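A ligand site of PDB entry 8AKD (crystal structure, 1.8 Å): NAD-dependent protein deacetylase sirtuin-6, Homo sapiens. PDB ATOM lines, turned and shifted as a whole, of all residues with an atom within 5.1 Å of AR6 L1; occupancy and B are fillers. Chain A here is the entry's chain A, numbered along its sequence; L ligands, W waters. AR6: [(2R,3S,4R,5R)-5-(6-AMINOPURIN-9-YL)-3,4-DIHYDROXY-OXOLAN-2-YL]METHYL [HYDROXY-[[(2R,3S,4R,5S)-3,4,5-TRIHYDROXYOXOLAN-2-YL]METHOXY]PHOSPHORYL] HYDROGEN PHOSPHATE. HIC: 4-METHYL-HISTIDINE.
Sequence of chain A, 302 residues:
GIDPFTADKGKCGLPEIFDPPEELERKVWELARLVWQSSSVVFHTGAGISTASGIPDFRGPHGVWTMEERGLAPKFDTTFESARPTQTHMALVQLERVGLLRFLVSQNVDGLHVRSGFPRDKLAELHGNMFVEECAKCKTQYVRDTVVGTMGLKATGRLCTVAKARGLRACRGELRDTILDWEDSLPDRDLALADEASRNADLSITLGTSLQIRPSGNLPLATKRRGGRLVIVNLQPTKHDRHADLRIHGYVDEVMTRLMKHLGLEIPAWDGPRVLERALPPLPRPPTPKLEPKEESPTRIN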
ATOM      1  N   GLU A  16     -30.869  26.590 -23.492  1.00  0.00           N
ATOM      2  CA  GLU A  16     -31.303  25.189 -23.218  1.00  0.00           C
ATOM      3  C   GLU A  16     -32.212  24.770 -24.369  1.00  0.00           C
ATOM      4  O   GLU A  16     -32.808  25.655 -25.025  1.00  0.00           O
ATOM      5  CB  GLU A  16     -31.934  25.083 -21.833  1.00  0.00           C
ATOM      6  CG  GLU A  16     -30.954  25.349 -20.704  1.00  0.00           C
ATOM      7  CD  GLU A  16     -31.525  25.023 -19.356  1.00  0.00           C
ATOM      8  OE1 GLU A  16     -32.752  25.270 -19.177  1.00  0.00           O
ATOM      9  OE2 GLU A  16     -30.790  24.450 -18.517  1.00  0.00           O
ATOM     10  N   GLY A  46     -21.262  14.041 -16.274  1.00  0.00           N
ATOM     11  CA  GLY A  46     -20.741  15.329 -15.849  1.00  0.00           C
ATOM     12  C   GLY A  46     -21.746  16.019 -14.949  1.00  0.00           C
ATOM     13  O   GLY A  46     -22.668  15.324 -14.506  1.00  0.00           O
ATOM     14  N   ALA A  47     -21.516  17.304 -14.712  1.00  0.00           N
ATOM     15  CA  ALA A  47     -22.109  18.055 -13.589  1.00  0.00           C
ATOM     16  C   ALA A  47     -23.637  18.092 -13.722  1.00  0.00           C
ATOM     17  O   ALA A  47     -24.268  18.225 -12.634  1.00  0.00           O
ATOM     18  CB  ALA A  47     -21.536  19.450 -13.490  1.00  0.00           C
ATOM     19  N   GLY A  48     -24.186  17.971 -14.930  1.00  0.00           N
ATOM     20  CA  GLY A  48     -25.659  18.049 -15.154  1.00  0.00           C
ATOM     21  C   GLY A  48     -26.414  16.949 -14.419  1.00  0.00           C
ATOM     22  O   GLY A  48     -27.617  17.140 -14.093  1.00  0.00           O
ATOM     23  N   THR A  51     -27.363  18.422 -10.629  1.00  0.00           N
ATOM     24  CA  THR A  51     -28.048  19.735 -10.563  1.00  0.00           C
ATOM     25  C   THR A  51     -29.363  19.504  -9.801  1.00  0.00           C
ATOM     26  O   THR A  51     -29.755  20.425  -9.063  1.00  0.00           O
ATOM     27  CB  THR A  51     -28.260  20.407 -11.917  1.00  0.00           C
ATOM     28  OG1 THR A  51     -29.008  19.585 -12.813  1.00  0.00           O
ATOM     29  CG2 THR A  51     -26.995  20.943 -12.569  1.00  0.00           C
ATOM     30  N   ASP A  57     -24.075  23.110 -11.900  1.00  0.00           N
ATOM     31  CA  ASP A  57     -23.064  22.698 -12.920  1.00  0.00           C
ATOM     32  C   ASP A  57     -22.085  23.851 -13.176  1.00  0.00           C
ATOM     33  O   ASP A  57     -22.070  24.827 -12.394  1.00  0.00           O
ATOM     34  CB  ASP A  57     -23.769  22.168 -14.167  1.00  0.00           C
ATOM     35  CG  ASP A  57     -24.657  23.165 -14.913  1.00  0.00           C
ATOM     36  OD1 ASP A  57     -24.479  24.398 -14.767  1.00  0.00           O
ATOM     37  OD2 ASP A  57     -25.527  22.677 -15.625  1.00  0.00           O
ATOM     38  N   PHE A  58     -21.250  23.760 -14.215  1.00  0.00           N
ATOM     39  CA  PHE A  58     -20.207  24.769 -14.537  1.00  0.00           C
ATOM     40  C   PHE A  58     -20.680  25.728 -15.663  1.00  0.00           C
ATOM     41  O   PHE A  58     -20.357  26.924 -15.555  1.00  0.00           O
ATOM     42  CB  PHE A  58     -18.908  24.051 -14.918  1.00  0.00           C
ATOM     43  CG  PHE A  58     -18.272  23.331 -13.767  1.00  0.00           C
ATOM     44  CD1 PHE A  58     -17.436  24.017 -12.895  1.00  0.00           C
ATOM     45  CD2 PHE A  58     -18.511  21.978 -13.519  1.00  0.00           C
ATOM     46  CE1 PHE A  58     -16.867  23.381 -11.809  1.00  0.00           C
ATOM     47  CE2 PHE A  58     -17.908  21.335 -12.456  1.00  0.00           C
ATOM     48  CZ  PHE A  58     -17.092  22.041 -11.591  1.00  0.00           C
ATOM     49  N   ARG A  59     -21.375  25.233 -16.696  1.00  0.00           N
ATOM     50  CA  ARG A  59     -21.641  25.950 -17.979  1.00  0.00           C
ATOM     51  C   ARG A  59     -23.141  26.055 -18.308  1.00  0.00           C
ATOM     52  O   ARG A  59     -23.471  26.645 -19.320  1.00  0.00           O
ATOM     53  CB  ARG A  59     -20.845  25.263 -19.099  1.00  0.00           C
ATOM     54  CG  ARG A  59     -19.348  25.409 -18.886  1.00  0.00           C
ATOM     55  CD  ARG A  59     -18.469  24.757 -19.961  1.00  0.00           C
ATOM     56  NE  ARG A  59     -17.103  24.728 -19.482  1.00  0.00           N
ATOM     57  CZ  ARG A  59     -16.528  23.757 -18.751  1.00  0.00           C
ATOM     58  NH1 ARG A  59     -17.184  22.645 -18.464  1.00  0.00           N
ATOM     59  NH2 ARG A  59     -15.286  23.895 -18.350  1.00  0.00           N
ATOM     60  N   GLY A  60     -24.032  25.561 -17.446  1.00  0.00           N
ATOM     61  CA  GLY A  60     -25.486  25.768 -17.588  1.00  0.00           C
ATOM     62  C   GLY A  60     -25.850  27.231 -17.343  1.00  0.00           C
ATOM     63  O   GLY A  60     -24.990  28.054 -17.005  1.00  0.00           O
ATOM     64  N   TRP A  65     -19.083  28.719 -13.763  1.00  0.00           N
ATOM     65  CA  TRP A  65     -18.345  29.607 -14.704  1.00  0.00           C
ATOM     66  C   TRP A  65     -19.288  30.616 -15.353  1.00  0.00           C
ATOM     67  O   TRP A  65     -18.890  31.788 -15.461  1.00  0.00           O
ATOM     68  CB  TRP A  65     -17.574  28.831 -15.779  1.00  0.00           C
ATOM     69  CG  TRP A  65     -16.668  27.754 -15.276  1.00  0.00           C
ATOM     70  CD1 TRP A  65     -16.446  26.574 -15.908  1.00  0.00           C
ATOM     71  CD2 TRP A  65     -15.875  27.724 -14.071  1.00  0.00           C
ATOM     72  NE1 TRP A  65     -15.571  25.809 -15.186  1.00  0.00           N
ATOM     73  CE2 TRP A  65     -15.208  26.483 -14.061  1.00  0.00           C
ATOM     74  CE3 TRP A  65     -15.656  28.612 -13.008  1.00  0.00           C
ATOM     75  CZ2 TRP A  65     -14.353  26.096 -13.025  1.00  0.00           C
ATOM     76  CZ3 TRP A  65     -14.812  28.241 -11.984  1.00  0.00           C
ATOM     77  CH2 TRP A  65     -14.166  27.002 -11.994  1.00  0.00           C
ATOM     78  N   GLN A 107     -16.603  13.019 -14.762  1.00  0.00           N
ATOM     79  CA  GLN A 107     -15.833  14.266 -14.644  1.00  0.00           C
ATOM     80  C   GLN A 107     -16.172  14.895 -13.303  1.00  0.00           C
ATOM     81  O   GLN A 107     -15.562  15.869 -12.974  1.00  0.00           O
ATOM     82  CB  GLN A 107     -16.196  15.158 -15.830  1.00  0.00           C
ATOM     83  CG  GLN A 107     -15.751  14.606 -17.185  1.00  0.00           C
ATOM     84  CD  GLN A 107     -16.160  15.515 -18.309  1.00  0.00           C
ATOM     85  OE1 GLN A 107     -15.621  16.607 -18.452  1.00  0.00           O
ATOM     86  NE2 GLN A 107     -17.177  15.101 -19.070  1.00  0.00           N
ATOM     87  N   ASN A 108     -17.128  14.331 -12.572  1.00  0.00           N
ATOM     88  CA  ASN A 108     -17.702  14.978 -11.369  1.00  0.00           C
ATOM     89  C   ASN A 108     -16.758  14.708 -10.192  1.00  0.00           C
ATOM     90  O   ASN A 108     -16.261  13.555 -10.069  1.00  0.00           O
ATOM     91  CB  ASN A 108     -19.121  14.481 -11.100  1.00  0.00           C
ATOM     92  CG  ASN A 108     -20.096  14.924 -12.164  1.00  0.00           C
ATOM     93  OD1 ASN A 108     -19.814  15.760 -13.009  1.00  0.00           O
ATOM     94  ND2 ASN A 108     -21.255  14.279 -12.190  1.00  0.00           N
ATOM     95  N   HIS A 127     -11.544  13.657 -12.767  1.00  0.00           N
ATOM     96  CA  HIS A 127     -11.230  14.997 -12.202  1.00  0.00           C
ATOM     97  C   HIS A 127     -11.031  14.892 -10.677  1.00  0.00           C
ATOM     98  O   HIS A 127     -10.766  15.934 -10.017  1.00  0.00           O
ATOM     99  CB  HIS A 127     -12.280  15.999 -12.697  1.00  0.00           C
ATOM    100  CG  HIS A 127     -12.326  16.099 -14.194  1.00  0.00           C
ATOM    101  ND1 HIS A 127     -13.314  16.814 -14.891  1.00  0.00           N
ATOM    102  CD2 HIS A 127     -11.496  15.597 -15.148  1.00  0.00           C
ATOM    103  CE1 HIS A 127     -13.103  16.721 -16.178  1.00  0.00           C
ATOM    104  NE2 HIS A 127     -11.958  15.997 -16.358  1.00  0.00           N
ATOM    105  N   TRP A 182      -6.389  23.036 -13.205  1.00  0.00           N
ATOM    106  CA  TRP A 182      -6.483  23.170 -14.680  1.00  0.00           C
ATOM    107  C   TRP A 182      -5.287  22.507 -15.398  1.00  0.00           C
ATOM    108  O   TRP A 182      -5.531  21.810 -16.400  1.00  0.00           O
ATOM    109  CB  TRP A 182      -6.621  24.643 -15.080  1.00  0.00           C
ATOM    110  CG  TRP A 182      -7.981  25.204 -14.799  1.00  0.00           C
ATOM    111  CD1 TRP A 182      -8.385  25.874 -13.679  1.00  0.00           C
ATOM    112  CD2 TRP A 182      -9.134  25.123 -15.653  1.00  0.00           C
ATOM    113  NE1 TRP A 182      -9.708  26.213 -13.778  1.00  0.00           N
ATOM    114  CE2 TRP A 182     -10.191  25.773 -14.978  1.00  0.00           C
ATOM    115  CE3 TRP A 182      -9.372  24.580 -16.921  1.00  0.00           C
ATOM    116  CZ2 TRP A 182     -11.467  25.875 -15.526  1.00  0.00           C
ATOM    117  CZ3 TRP A 182     -10.635  24.685 -17.467  1.00  0.00           C
ATOM    118  CH2 TRP A 182     -11.671  25.333 -16.771  1.00  0.00           C
ATOM    119  N   GLY A 208     -25.604  14.856 -18.855  1.00  0.00           N
ATOM    120  CA  GLY A 208     -25.271  16.186 -18.315  1.00  0.00           C
ATOM    121  C   GLY A 208     -23.798  16.512 -18.354  1.00  0.00           C
ATOM    122  O   GLY A 208     -23.297  16.848 -17.326  1.00  0.00           O
ATOM    123  N   THR A 209     -23.130  16.333 -19.498  1.00  0.00           N
ATOM    124  CA  THR A 209     -21.804  16.909 -19.780  1.00  0.00           C
ATOM    125  C   THR A 209     -21.893  17.643 -21.125  1.00  0.00           C
ATOM    126  O   THR A 209     -22.490  17.104 -22.063  1.00  0.00           O
ATOM    127  CB  THR A 209     -20.693  15.849 -19.754  1.00  0.00           C
ATOM    128  OG1 THR A 209     -19.497  16.552 -20.094  1.00  0.00           O
ATOM    129  CG2 THR A 209     -20.917  14.708 -20.690  1.00  0.00           C
ATOM    130  N   SER A 210     -21.289  18.830 -21.208  1.00  0.00           N
ATOM    131  CA  SER A 210     -21.147  19.625 -22.439  1.00  0.00           C
ATOM    132  C   SER A 210     -19.949  19.106 -23.272  1.00  0.00           C
ATOM    133  O   SER A 210     -19.800  19.604 -24.389  1.00  0.00           O
ATOM    134  CB  SER A 210     -21.066  21.127 -22.129  1.00  0.00           C
ATOM    135  OG  SER A 210     -19.864  21.481 -21.471  1.00  0.00           O
ATOM    136  N   LEU A 211     -19.109  18.216 -22.719  1.00  0.00           N
ATOM    137  CA  LEU A 211     -18.013  17.495 -23.473  1.00  0.00           C
ATOM    138  C   LEU A 211     -16.934  18.462 -24.008  1.00  0.00           C
ATOM    139  O   LEU A 211     -16.321  18.159 -25.066  1.00  0.00           O
ATOM    140  CB  LEU A 211     -18.622  16.705 -24.625  1.00  0.00           C
ATOM    141  CG  LEU A 211     -19.653  15.651 -24.237  1.00  0.00           C
ATOM    142  CD1 LEU A 211     -20.439  15.168 -25.446  1.00  0.00           C
ATOM    143  CD2 LEU A 211     -19.001  14.467 -23.513  1.00  0.00           C
ATOM    144  N   GLN A 212     -16.669  19.539 -23.279  1.00  0.00           N
ATOM    145  CA  GLN A 212     -15.770  20.657 -23.699  1.00  0.00           C
ATOM    146  C   GLN A 212     -14.348  20.444 -23.148  1.00  0.00           C
ATOM    147  O   GLN A 212     -13.455  21.212 -23.563  1.00  0.00           O
ATOM    148  CB  GLN A 212     -16.305  21.991 -23.210  1.00  0.00           C
ATOM    149  CG  GLN A 212     -17.598  22.400 -23.876  1.00  0.00           C
ATOM    150  CD  GLN A 212     -17.938  23.853 -23.644  1.00  0.00           C
ATOM    151  OE1 GLN A 212     -17.121  24.746 -23.876  1.00  0.00           O
ATOM    152  NE2 GLN A 212     -19.180  24.109 -23.230  1.00  0.00           N
ATOM    153  N   ILE A 213     -14.130  19.494 -22.244  1.00  0.00           N
ATOM    154  CA  ILE A 213     -12.824  19.282 -21.542  1.00  0.00           C
ATOM    155  C   ILE A 213     -12.152  18.050 -22.147  1.00  0.00           C
ATOM    156  O   ILE A 213     -12.750  16.963 -22.086  1.00  0.00           O
ATOM    157  CB  ILE A 213     -13.035  19.177 -20.014  1.00  0.00           C
ATOM    158  CG1 ILE A 213     -13.339  20.533 -19.379  1.00  0.00           C
ATOM    159  CG2 ILE A 213     -11.851  18.504 -19.335  1.00  0.00           C
ATOM    160  CD1 ILE A 213     -12.151  21.458 -19.250  1.00  0.00           C
ATOM    161  N   VAL A 233     -27.232  12.871 -23.967  1.00  0.00           N
ATOM    162  CA  VAL A 233     -28.379  13.439 -23.192  1.00  0.00           C
ATOM    163  C   VAL A 233     -27.846  14.711 -22.504  1.00  0.00           C
ATOM    164  O   VAL A 233     -26.945  14.650 -21.618  1.00  0.00           O
ATOM    165  CB  VAL A 233     -28.966  12.407 -22.210  1.00  0.00           C
ATOM    166  CG1 VAL A 233     -30.239  12.968 -21.570  1.00  0.00           C
ATOM    167  CG2 VAL A 233     -29.230  11.039 -22.845  1.00  0.00           C
ATOM    168  N   ASN A 234     -28.404  15.864 -22.856  1.00  0.00           N
ATOM    169  CA  ASN A 234     -27.962  17.178 -22.345  1.00  0.00           C
ATOM    170  C   ASN A 234     -29.038  18.204 -22.670  1.00  0.00           C
ATOM    171  O   ASN A 234     -29.602  18.175 -23.811  1.00  0.00           O
ATOM    172  CB  ASN A 234     -26.618  17.637 -22.915  1.00  0.00           C
ATOM    173  CG  ASN A 234     -25.773  18.421 -21.932  1.00  0.00           C
ATOM    174  OD1 ASN A 234     -25.427  17.920 -20.859  1.00  0.00           O
ATOM    175  ND2 ASN A 234     -25.385  19.627 -22.288  1.00  0.00           N
ATOM    176  N   LEU A 235     -29.260  19.147 -21.764  1.00  0.00           N
ATOM    177  CA  LEU A 235     -30.178  20.273 -22.012  1.00  0.00           C
ATOM    178  C   LEU A 235     -29.574  21.254 -23.040  1.00  0.00           C
ATOM    179  O   LEU A 235     -30.339  21.750 -23.902  1.00  0.00           O
ATOM    180  CB  LEU A 235     -30.480  20.930 -20.666  1.00  0.00           C
ATOM    181  CG  LEU A 235     -31.544  20.186 -19.862  1.00  0.00           C
ATOM    182  CD1 LEU A 235     -31.665  20.778 -18.476  1.00  0.00           C
ATOM    183  CD2 LEU A 235     -32.866  20.195 -20.628  1.00  0.00           C
ATOM    184  N   GLN A 236     -28.278  21.509 -22.944  1.00  0.00           N
ATOM    185  CA  GLN A 236     -27.544  22.478 -23.815  1.00  0.00           C
ATOM    186  C   GLN A 236     -26.898  21.693 -24.946  1.00  0.00           C
ATOM    187  O   GLN A 236     -26.752  20.486 -24.849  1.00  0.00           O
ATOM    188  CB  GLN A 236     -26.426  23.183 -23.056  1.00  0.00           C
ATOM    189  CG  GLN A 236     -26.858  24.325 -22.164  1.00  0.00           C
ATOM    190  CD  GLN A 236     -25.729  24.921 -21.368  1.00  0.00           C
ATOM    191  OE1 GLN A 236     -24.733  24.285 -21.015  1.00  0.00           O
ATOM    192  NE2 GLN A 236     -25.871  26.192 -21.013  1.00  0.00           N
ATOM    193  N   PRO A 237     -26.460  22.395 -26.020  1.00  0.00           N
ATOM    194  CA  PRO A 237     -25.557  21.789 -27.006  1.00  0.00           C
ATOM    195  C   PRO A 237     -24.270  21.296 -26.358  1.00  0.00           C
ATOM    196  O   PRO A 237     -23.876  21.804 -25.353  1.00  0.00           O
ATOM    197  CB  PRO A 237     -25.245  22.973 -27.953  1.00  0.00           C
ATOM    198  CG  PRO A 237     -26.467  23.821 -27.841  1.00  0.00           C
ATOM    199  CD  PRO A 237     -26.845  23.763 -26.383  1.00  0.00           C
ATOM    200  N   GLY A 250     -33.481  17.108 -22.585  1.00  0.00           N
ATOM    201  CA  GLY A 250     -34.447  16.866 -21.496  1.00  0.00           C
ATOM    202  C   GLY A 250     -33.713  16.714 -20.190  1.00  0.00           C
ATOM    203  O   GLY A 250     -32.463  16.651 -20.227  1.00  0.00           O
ATOM    204  N   TYR A 251     -34.414  16.741 -19.065  1.00  0.00           N
ATOM    205  CA  TYR A 251     -33.794  16.545 -17.740  1.00  0.00           C
ATOM    206  C   TYR A 251     -33.341  15.084 -17.651  1.00  0.00           C
ATOM    207  O   TYR A 251     -34.120  14.170 -18.065  1.00  0.00           O
ATOM    208  CB  TYR A 251     -34.762  16.990 -16.632  1.00  0.00           C
ATOM    209  CG  TYR A 251     -35.076  18.457 -16.655  1.00  0.00           C
ATOM    210  CD1 TYR A 251     -34.272  19.364 -15.985  1.00  0.00           C
ATOM    211  CD2 TYR A 251     -36.159  18.950 -17.370  1.00  0.00           C
ATOM    212  CE1 TYR A 251     -34.545  20.719 -15.978  1.00  0.00           C
ATOM    213  CE2 TYR A 251     -36.437  20.307 -17.400  1.00  0.00           C
ATOM    214  CZ  TYR A 251     -35.630  21.188 -16.700  1.00  0.00           C
ATOM    215  OH  TYR A 251     -35.894  22.519 -16.728  1.00  0.00           O
ATOM    216  N   VAL A 252     -32.098  14.857 -17.194  1.00  0.00           N
ATOM    217  CA  VAL A 252     -31.528  13.475 -17.171  1.00  0.00           C
ATOM    218  C   VAL A 252     -32.382  12.575 -16.292  1.00  0.00           C
ATOM    219  O   VAL A 252     -32.590  11.456 -16.693  1.00  0.00           O
ATOM    220  CB  VAL A 252     -30.034  13.444 -16.817  1.00  0.00           C
ATOM    221  CG1 VAL A 252     -29.210  13.957 -17.986  1.00  0.00           C
ATOM    222  CG2 VAL A 252     -29.695  14.192 -15.533  1.00  0.00           C
HETATM  223  N1  AR6 L   1     -30.564  17.305 -17.181  1.00  0.00           N
HETATM  224  C2  AR6 L   1     -29.844  17.348 -18.302  1.00  0.00           C
HETATM  225  N3  AR6 L   1     -28.785  18.111 -18.585  1.00  0.00           N
HETATM  226  C4  AR6 L   1     -28.467  18.909 -17.559  1.00  0.00           C
HETATM  227  C5  AR6 L   1     -29.123  18.989 -16.356  1.00  0.00           C
HETATM  228  C6  AR6 L   1     -30.219  18.110 -16.153  1.00  0.00           C
HETATM  229  N6  AR6 L   1     -30.945  18.097 -15.047  1.00  0.00           N
HETATM  230  N7  AR6 L   1     -28.498  19.918 -15.537  1.00  0.00           N
HETATM  231  C8  AR6 L   1     -27.517  20.410 -16.255  1.00  0.00           C
HETATM  232  N9  AR6 L   1     -27.463  19.833 -17.498  1.00  0.00           N
HETATM  233  PA  AR6 L   1     -20.770  21.438 -17.769  1.00  0.00           P
HETATM  234  PB  AR6 L   1     -19.103  19.084 -17.299  1.00  0.00           P
HETATM  235  C1' AR6 L   1     -26.488  20.057 -18.551  1.00  0.00           C
HETATM  236  O1A AR6 L   1     -19.794  21.912 -18.806  1.00  0.00           O
HETATM  237  O1B AR6 L   1     -19.248  17.997 -16.279  1.00  0.00           O
HETATM  238  C1D AR6 L   1     -15.254  21.941 -15.316  1.00  0.00           C
HETATM  239  O1D AR6 L   1     -14.187  22.871 -15.325  1.00  0.00           O
HETATM  240  C2' AR6 L   1     -26.137  21.492 -18.904  1.00  0.00           C
HETATM  241  O2' AR6 L   1     -26.870  21.972 -20.008  1.00  0.00           O
HETATM  242  O2A AR6 L   1     -21.357  22.426 -16.829  1.00  0.00           O
HETATM  243  O2B AR6 L   1     -19.296  18.761 -18.729  1.00  0.00           O
HETATM  244  C2D AR6 L   1     -14.944  20.824 -14.302  1.00  0.00           C
HETATM  245  O2D AR6 L   1     -13.564  20.510 -14.176  1.00  0.00           O
HETATM  246  C3' AR6 L   1     -24.645  21.373 -19.301  1.00  0.00           C
HETATM  247  O3' AR6 L   1     -24.606  21.503 -20.691  1.00  0.00           O
HETATM  248  O3A AR6 L   1     -20.092  20.292 -16.870  1.00  0.00           O
HETATM  249  C3D AR6 L   1     -15.740  19.650 -14.858  1.00  0.00           C
HETATM  250  O3D AR6 L   1     -15.354  18.369 -14.341  1.00  0.00           O
HETATM  251  C4' AR6 L   1     -24.202  20.009 -18.769  1.00  0.00           C
HETATM  252  O4' AR6 L   1     -25.333  19.442 -18.056  1.00  0.00           O
HETATM  253  C4D AR6 L   1     -15.468  19.823 -16.362  1.00  0.00           C
HETATM  254  O4D AR6 L   1     -15.406  21.259 -16.583  1.00  0.00           O
HETATM  255  C5' AR6 L   1     -23.059  20.119 -17.809  1.00  0.00           C
HETATM  256  O5' AR6 L   1     -21.963  20.745 -18.547  1.00  0.00           O
HETATM  257  C5D AR6 L   1     -16.485  19.202 -17.274  1.00  0.00           C
HETATM  258  O5D AR6 L   1     -17.755  19.875 -17.095  1.00  0.00           O
HETATM  259  N   HIC L   2      -7.140  18.860 -20.197  1.00  0.00           N
HETATM  260  CA  HIC L   2      -6.439  18.533 -18.916  1.00  0.00           C
HETATM  261  C   HIC L   2      -5.058  17.925 -19.215  1.00  0.00           C
HETATM  262  O   HIC L   2      -4.973  16.819 -19.751  1.00  0.00           O
HETATM  263  CB  HIC L   2      -7.269  17.576 -18.063  1.00  0.00           C
HETATM  264  CG  HIC L   2      -8.024  18.252 -16.969  1.00  0.00           C
HETATM  265  ND1 HIC L   2      -7.385  18.673 -15.821  1.00  0.00           N
HETATM  266  CD2 HIC L   2      -9.359  18.552 -16.889  1.00  0.00           C
HETATM  267  CE1 HIC L   2      -8.320  19.222 -15.077  1.00  0.00           C
HETATM  268  NE2 HIC L   2      -9.548  19.180 -15.676  1.00  0.00           N
HETATM  269  CZ  HIC L   2     -10.836  19.680 -15.191  1.00  0.00           C
HETATM  270  OXT HIC L   2      -4.035  18.525 -18.918  1.00  0.00           O
HETATM  271  O   HOH W   1     -27.860  23.846 -15.895  1.00  0.00           O
HETATM  272  O   HOH W   2     -17.736  20.332 -20.560  1.00  0.00           O
HETATM  273  O   HOH W   3     -32.276  15.492 -13.856  1.00  0.00           O
HETATM  274  O   HOH W   4     -29.732  16.505 -12.351  1.00  0.00           O
HETATM  275  O   HOH W   5     -17.952  17.651 -13.823  1.00  0.00           O
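N of Arg 59 lies within hydrogen-bond range of O2A of AR6 L1. The backbone NH (N) of Gln 236 sits close to an oxygen (O2') of AR6 L1. A ring nitrogen (ND1) of His 127 is in hydrogen-bond range of an oxygen (O3D) of AR6 L1. OG1 of Thr 51 lies within hydrogen-bond range of N7 of AR6 L1, at 2.8 Å. N1 of AR6 L1 sits at hydrogen-bond distance from N of Val 252, at 2.9 Å. OE1 of Gln 236 is in hydrogen-bond range of O3' of AR6 L1 (2.8 Å). N of Phe 58 sits at hydrogen-bond distance from O2A of AR6 L1 (2.9 Å). An oxygen (O1D) of AR6 L1 lies within hydrogen-bond range of the indole nitrogen of Trp 65, 3.3 Å away. An oxygen (O2B) of AR6 L1 lies within hydrogen-bond range of the backbone NH (N) of Ser 210, at 3.2 Å. OG1 of Thr 209 is in hydrogen-bond range of O2B of AR6 L1, 2.6 Å away. O1B of AR6 L1 is in hydrogen-bond range of N of Ala 47 (2.8 Å). O1A of AR6 L1 lies within salt-bridge range of NH1 of Arg 59. The backbone NH (N) of Leu 235 sits at hydrogen-bond distance from a nitrogen (N3) of AR6 L1, at 3.4 Å. O1A of AR6 L1 is in hydrogen-bond range of OG of Ser 210, 2.7 Å away. The side-chain amide nitrogen (ND2) of Asn 234 sits at hydrogen-bond distance from an oxygen (O3') of AR6 L1. The backbone carbonyl oxygen of Gln 107 sits at hydrogen-bond distance from an oxygen (O3D) of AR6 L1.
The side-chain amide nitrogen (ND2) of Asn 234 is in hydrogen-bond range of the backbone carbonyl oxygen (O) of Gln 236 (3.0 Å). N of Ala 47 is in hydrogen-bond range of OD1 of Asn 108. OG of Ser 210 sits at hydrogen-bond distance from NE2 of Gln 212, 3.2 Å away. N of Leu 211 sits at hydrogen-bond distance from OG1 of Thr 209 (3.1 Å). The backbone NH of Thr 209 sits at hydrogen-bond distance from the side-chain amide oxygen of Asn 234, 3.1 Å away. The side-chain amide nitrogen (ND2) of Asn 108 lies within hydrogen-bond range of the backbone carbonyl oxygen (O) of Gly 46 (2.9 Å). O of Gln 107 lies within hydrogen-bond range of ND1 of His 127, 3.1 Å away. N of Ala 47 is in hydrogen-bond range of O of Gly 208, at 3.2 Å.
O of Gly 48 sits close to N7 of AR6 L1. An oxygen (O4') of AR6 L1 sits close to the backbone carbonyl oxygen (O) of Gly 208. CA of Gly 46 touches O1B of AR6 L1, at 3.1 Å. OD2 of Asp 57 touches C8 of AR6 L1, at 3.1 Å. Trp 182 touches AR6 L1. Ile 213 touches AR6 L1. O of Gly 250 touches C2 of AR6 L1, at 3.3 Å. Tyr 251 touches AR6 L1. Hydrophobic or aromatic side chains that line AR6 L1: Ala 47, Phe 58, Trp 65, His 127, Trp 182, Ile 213, Leu 235, Tyr 251 and Val 252. 21 residues have an atom within 4 Å of AR6 L1: Gly 46, Ala 47, Gly 48, Thr 51, Asp 57, Phe 58, Arg 59, Trp 65, Gln 107, His 127, Trp 182, Gly 208, Thr 209, Ser 210, Ile 213, Asn 234, Leu 235, Gln 236, Gly 250, Tyr 251 and Val 252.
Water W5 lies within hydrogen-bond range of an oxygen (O3D) of AR6 L1 (2.7 Å), the side-chain amide oxygen of Asn 108 (2.8 Å) and the backbone carbonyl oxygen of Gln 107 (3.1 Å). Water W3 lies within hydrogen-bond range of N6 of AR6 L1 (3.2 Å) and N of Val 252 (3.4 Å). Water W4 lies within hydrogen-bond range of the backbone carbonyl oxygen of Gly 48, the side-chain hydroxyl of Thr 51 and a nitrogen (N6) of AR6 L1.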
